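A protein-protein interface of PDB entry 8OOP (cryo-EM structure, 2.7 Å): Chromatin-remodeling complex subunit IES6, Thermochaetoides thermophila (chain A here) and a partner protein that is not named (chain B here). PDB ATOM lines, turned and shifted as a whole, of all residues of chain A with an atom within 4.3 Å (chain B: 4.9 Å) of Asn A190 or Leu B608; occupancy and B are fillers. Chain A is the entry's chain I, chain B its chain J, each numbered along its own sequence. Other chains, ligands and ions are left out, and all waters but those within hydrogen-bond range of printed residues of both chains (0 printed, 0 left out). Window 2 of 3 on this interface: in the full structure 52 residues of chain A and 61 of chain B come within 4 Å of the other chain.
The side-chain carboxylate (OE2) of Glu A192 is in hydrogen-bond range of the backbone NH (N) of Leu B609, 2.8 Å away. The backbone NH of Leu B608 lies within hydrogen-bond range of the side-chain carboxylate of Glu A192 (2.9 Å).
OD1 of Asn A190 lies within hydrogen-bond range of N of Ile A193 (3.0 Å). The backbone NH (N) of Glu A192 lies within hydrogen-bond range of the side-chain amide oxygen (OD1) of Asn A190 (3.2 Å). The side-chain hydroxyl of Ser B607 sits close to the backbone NH of His B610, at 3.4 Å.
His A189 touches Leu B608. Leu B608 touches Asn A190. OE2 of Glu A192 touches CB of Ser B607 (3.6 Å). CD1 of Ile A193 touches CD2 of Leu B608 (3.7 Å).
Asn A190 touches just one residue of chain B: Leu B608. Leu B608 touches just these residues of chain A: His A189, Asn A190, Glu A192 and Ile A193. Printed residues of chain A within 4 Å of Leu B609: Glu A192 (2.8 Å). Of the printed residues of chain B, Glu A192 touches Ser B607 (3.6 Å), Leu B608 (2.9 Å) and Leu B609 (2.8 Å). Of the printed residues of chain A, Ser B607 touches Glu A192 (3.6 Å). Of the printed residues of chain B, Ile A193 touches Leu B608. The nearest printed residue of chain B that does not touch Asn A190 is Leu B609 (6.8 Å).
Printed residues of chain B that touch a printed residue of chain A: Ser B607, Leu B608 and Leu B609. Hydrophobic or aromatic side chains of chain A that line the printed part of chain B: His A189 and Ile A193. Among the printed residues, 6 pairs touch across the chains. Among the printed residues, no Asp or Glu carboxylate lies within 4 Å of a Lys or Arg side-chain nitrogen of the other chain.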
ATOM      1  N   TYR A 188     -15.827 -17.152 -28.722  1.00  0.00           N
ATOM      2  CA  TYR A 188     -14.581 -17.269 -27.975  1.00  0.00           C
ATOM      3  C   TYR A 188     -13.876 -18.591 -28.242  1.00  0.00           C
ATOM      4  O   TYR A 188     -14.501 -19.597 -28.583  1.00  0.00           O
ATOM      5  CB  TYR A 188     -14.838 -17.062 -26.479  1.00  0.00           C
ATOM      6  CG  TYR A 188     -15.748 -18.089 -25.862  1.00  0.00           C
ATOM      7  CD1 TYR A 188     -17.114 -17.894 -25.874  1.00  0.00           C
ATOM      8  CD2 TYR A 188     -15.260 -19.244 -25.272  1.00  0.00           C
ATOM      9  CE1 TYR A 188     -17.977 -18.801 -25.319  1.00  0.00           C
ATOM     10  CE2 TYR A 188     -16.126 -20.175 -24.713  1.00  0.00           C
ATOM     11  CZ  TYR A 188     -17.485 -19.940 -24.737  1.00  0.00           C
ATOM     12  OH  TYR A 188     -18.373 -20.843 -24.204  1.00  0.00           O
ATOM     13  N   HIS A 189     -12.554 -18.554 -28.063  1.00  0.00           N
ATOM     14  CA  HIS A 189     -11.665 -19.662 -28.386  1.00  0.00           C
ATOM     15  C   HIS A 189     -11.659 -20.756 -27.320  1.00  0.00           C
ATOM     16  O   HIS A 189     -11.709 -21.944 -27.661  1.00  0.00           O
ATOM     17  CB  HIS A 189     -10.253 -19.108 -28.595  1.00  0.00           C
ATOM     18  CG  HIS A 189      -9.235 -20.132 -28.987  1.00  0.00           C
ATOM     19  ND1 HIS A 189      -9.307 -20.847 -30.160  1.00  0.00           N
ATOM     20  CD2 HIS A 189      -8.092 -20.527 -28.378  1.00  0.00           C
ATOM     21  CE1 HIS A 189      -8.270 -21.659 -30.245  1.00  0.00           C
ATOM     22  NE2 HIS A 189      -7.517 -21.484 -29.176  1.00  0.00           N
ATOM     23  N   ASN A 190     -11.608 -20.394 -26.041  1.00  0.00           N
ATOM     24  CA  ASN A 190     -11.344 -21.380 -24.997  1.00  0.00           C
ATOM     25  C   ASN A 190     -11.839 -20.863 -23.651  1.00  0.00           C
ATOM     26  O   ASN A 190     -12.302 -19.725 -23.529  1.00  0.00           O
ATOM     27  CB  ASN A 190      -9.855 -21.759 -24.984  1.00  0.00           C
ATOM     28  CG  ASN A 190      -8.948 -20.632 -24.525  1.00  0.00           C
ATOM     29  OD1 ASN A 190      -9.401 -19.564 -24.131  1.00  0.00           O
ATOM     30  ND2 ASN A 190      -7.646 -20.871 -24.589  1.00  0.00           N
ATOM     31  N   LYS A 191     -11.738 -21.732 -22.639  1.00  0.00           N
ATOM     32  CA  LYS A 191     -12.147 -21.416 -21.271  1.00  0.00           C
ATOM     33  C   LYS A 191     -11.437 -20.200 -20.685  1.00  0.00           C
ATOM     34  O   LYS A 191     -12.013 -19.501 -19.845  1.00  0.00           O
ATOM     35  CB  LYS A 191     -11.931 -22.642 -20.381  1.00  0.00           C
ATOM     36  CG  LYS A 191     -10.495 -23.133 -20.313  1.00  0.00           C
ATOM     37  CD  LYS A 191     -10.408 -24.450 -19.558  1.00  0.00           C
ATOM     38  CE  LYS A 191     -10.503 -24.231 -18.063  1.00  0.00           C
ATOM     39  NZ  LYS A 191      -9.236 -23.675 -17.512  1.00  0.00           N
ATOM     40  N   GLU A 192     -10.189 -19.942 -21.081  1.00  0.00           N
ATOM     41  CA  GLU A 192      -9.498 -18.752 -20.588  1.00  0.00           C
ATOM     42  C   GLU A 192     -10.165 -17.464 -21.061  1.00  0.00           C
ATOM     43  O   GLU A 192     -10.321 -16.517 -20.282  1.00  0.00           O
ATOM     44  CB  GLU A 192      -8.038 -18.774 -21.024  1.00  0.00           C
ATOM     45  CG  GLU A 192      -7.262 -17.528 -20.636  1.00  0.00           C
ATOM     46  CD  GLU A 192      -5.793 -17.642 -20.970  1.00  0.00           C
ATOM     47  OE1 GLU A 192      -5.286 -18.781 -21.027  1.00  0.00           O
ATOM     48  OE2 GLU A 192      -5.145 -16.597 -21.179  1.00  0.00           O
ATOM     49  N   ILE A 193     -10.555 -17.408 -22.332  1.00  0.00           N
ATOM     50  CA  ILE A 193     -11.202 -16.224 -22.886  1.00  0.00           C
ATOM     51  C   ILE A 193     -12.672 -16.121 -22.477  1.00  0.00           C
ATOM     52  O   ILE A 193     -13.203 -15.014 -22.350  1.00  0.00           O
ATOM     53  CB  ILE A 193     -11.006 -16.228 -24.412  1.00  0.00           C
ATOM     54  CG1 ILE A 193      -9.532 -15.957 -24.714  1.00  0.00           C
ATOM     55  CG2 ILE A 193     -11.901 -15.210 -25.099  1.00  0.00           C
ATOM     56  CD1 ILE A 193      -9.068 -16.439 -26.051  1.00  0.00           C
ATOM     57  N   PHE A 194     -13.344 -17.248 -22.250  1.00  0.00           N
ATOM     58  CA  PHE A 194     -14.659 -17.194 -21.616  1.00  0.00           C
ATOM     59  C   PHE A 194     -14.591 -16.568 -20.226  1.00  0.00           C
ATOM     60  O   PHE A 194     -15.490 -15.816 -19.835  1.00  0.00           O
ATOM     61  CB  PHE A 194     -15.263 -18.596 -21.538  1.00  0.00           C
ATOM     62  CG  PHE A 194     -16.644 -18.624 -20.948  1.00  0.00           C
ATOM     63  CD1 PHE A 194     -17.754 -18.407 -21.741  1.00  0.00           C
ATOM     64  CD2 PHE A 194     -16.832 -18.852 -19.595  1.00  0.00           C
ATOM     65  CE1 PHE A 194     -19.024 -18.420 -21.200  1.00  0.00           C
ATOM     66  CE2 PHE A 194     -18.097 -18.868 -19.050  1.00  0.00           C
ATOM     67  CZ  PHE A 194     -19.194 -18.647 -19.852  1.00  0.00           C
ATOM     68  N   LEU B 285      -0.581 -18.022 -32.014  1.00  0.00           N
ATOM     69  CA  LEU B 285      -0.223 -17.650 -30.648  1.00  0.00           C
ATOM     70  C   LEU B 285       0.487 -18.749 -29.862  1.00  0.00           C
ATOM     71  O   LEU B 285       0.717 -18.573 -28.662  1.00  0.00           O
ATOM     72  CB  LEU B 285      -1.465 -17.186 -29.885  1.00  0.00           C
ATOM     73  CG  LEU B 285      -2.062 -15.880 -30.409  1.00  0.00           C
ATOM     74  CD1 LEU B 285      -3.294 -15.491 -29.620  1.00  0.00           C
ATOM     75  CD2 LEU B 285      -1.010 -14.779 -30.349  1.00  0.00           C
ATOM     76  N   LYS B 606       1.894 -19.887 -18.961  1.00  0.00           N
ATOM     77  CA  LYS B 606       0.947 -20.901 -19.400  1.00  0.00           C
ATOM     78  C   LYS B 606      -0.359 -20.310 -19.923  1.00  0.00           C
ATOM     79  O   LYS B 606      -1.217 -21.063 -20.393  1.00  0.00           O
ATOM     80  CB  LYS B 606       0.650 -21.873 -18.252  1.00  0.00           C
ATOM     81  CG  LYS B 606       1.865 -22.650 -17.758  1.00  0.00           C
ATOM     82  CD  LYS B 606       2.472 -23.549 -18.824  1.00  0.00           C
ATOM     83  CE  LYS B 606       3.499 -24.494 -18.205  1.00  0.00           C
ATOM     84  NZ  LYS B 606       4.099 -25.430 -19.195  1.00  0.00           N
ATOM     85  N   SER B 607      -0.529 -18.991 -19.856  1.00  0.00           N
ATOM     86  CA  SER B 607      -1.726 -18.335 -20.360  1.00  0.00           C
ATOM     87  C   SER B 607      -1.652 -18.112 -21.870  1.00  0.00           C
ATOM     88  O   SER B 607      -0.601 -18.243 -22.502  1.00  0.00           O
ATOM     89  CB  SER B 607      -1.944 -17.001 -19.654  1.00  0.00           C
ATOM     90  OG  SER B 607      -1.076 -16.016 -20.174  1.00  0.00           O
ATOM     91  N   LEU B 608      -2.803 -17.753 -22.439  1.00  0.00           N
ATOM     92  CA  LEU B 608      -2.945 -17.339 -23.829  1.00  0.00           C
ATOM     93  C   LEU B 608      -3.011 -15.828 -24.006  1.00  0.00           C
ATOM     94  O   LEU B 608      -2.405 -15.296 -24.938  1.00  0.00           O
ATOM     95  CB  LEU B 608      -4.200 -17.981 -24.429  1.00  0.00           C
ATOM     96  CG  LEU B 608      -4.626 -17.625 -25.851  1.00  0.00           C
ATOM     97  CD1 LEU B 608      -3.535 -17.974 -26.845  1.00  0.00           C
ATOM     98  CD2 LEU B 608      -5.916 -18.352 -26.188  1.00  0.00           C
ATOM     99  N   LEU B 609      -3.729 -15.126 -23.126  1.00  0.00           N
ATOM    100  CA  LEU B 609      -3.904 -13.683 -23.265  1.00  0.00           C
ATOM    101  C   LEU B 609      -2.612 -12.909 -23.031  1.00  0.00           C
ATOM    102  O   LEU B 609      -2.466 -11.794 -23.544  1.00  0.00           O
ATOM    103  CB  LEU B 609      -5.001 -13.194 -22.327  1.00  0.00           C
ATOM    104  CG  LEU B 609      -6.390 -13.601 -22.806  1.00  0.00           C
ATOM    105  CD1 LEU B 609      -7.418 -13.423 -21.714  1.00  0.00           C
ATOM    106  CD2 LEU B 609      -6.749 -12.776 -24.035  1.00  0.00           C
ATOM    107  N   HIS B 610      -1.673 -13.464 -22.263  1.00  0.00           N
ATOM    108  CA  HIS B 610      -0.351 -12.851 -22.188  1.00  0.00           C
ATOM    109  C   HIS B 610       0.393 -12.952 -23.512  1.00  0.00           C
ATOM    110  O   HIS B 610       1.036 -11.986 -23.940  1.00  0.00           O
ATOM    111  CB  HIS B 610       0.468 -13.496 -21.073  1.00  0.00           C
ATOM    112  CG  HIS B 610       1.739 -12.771 -20.766  1.00  0.00           C
ATOM    113  ND1 HIS B 610       1.884 -11.935 -19.682  1.00  0.00           N
ATOM    114  CD2 HIS B 610       2.933 -12.764 -21.405  1.00  0.00           C
ATOM    115  CE1 HIS B 610       3.107 -11.439 -19.671  1.00  0.00           C
ATOM    116  NE2 HIS B 610       3.765 -11.926 -20.705  1.00  0.00           N
ATOM    117  N   ALA B 611       0.329 -14.110 -24.168  1.00  0.00           N
ATOM    118  CA  ALA B 611       0.935 -14.248 -25.487  1.00  0.00           C
ATOM    119  C   ALA B 611       0.308 -13.282 -26.482  1.00  0.00           C
ATOM    120  O   ALA B 611       1.009 -12.639 -27.270  1.00  0.00           O
ATOM    121  CB  ALA B 611       0.795 -15.685 -25.980  1.00  0.00           C
ATOM    122  N   PHE B 612      -1.019 -13.176 -26.452  1.00  0.00           N
ATOM    123  CA  PHE B 612      -1.738 -12.224 -27.291  1.00  0.00           C
ATOM    124  C   PHE B 612      -1.293 -10.784 -27.038  1.00  0.00           C
ATOM    125  O   PHE B 612      -0.981 -10.050 -27.982  1.00  0.00           O
ATOM    126  CB  PHE B 612      -3.235 -12.412 -27.033  1.00  0.00           C
ATOM    127  CG  PHE B 612      -4.132 -11.508 -27.822  1.00  0.00           C
ATOM    128  CD1 PHE B 612      -4.081 -11.483 -29.202  1.00  0.00           C
ATOM    129  CD2 PHE B 612      -5.087 -10.734 -27.180  1.00  0.00           C
ATOM    130  CE1 PHE B 612      -4.929 -10.672 -29.926  1.00  0.00           C
ATOM    131  CE2 PHE B 612      -5.939  -9.921 -27.901  1.00  0.00           C
ATOM    132  CZ  PHE B 612      -5.862  -9.893 -29.273  1.00  0.00           C
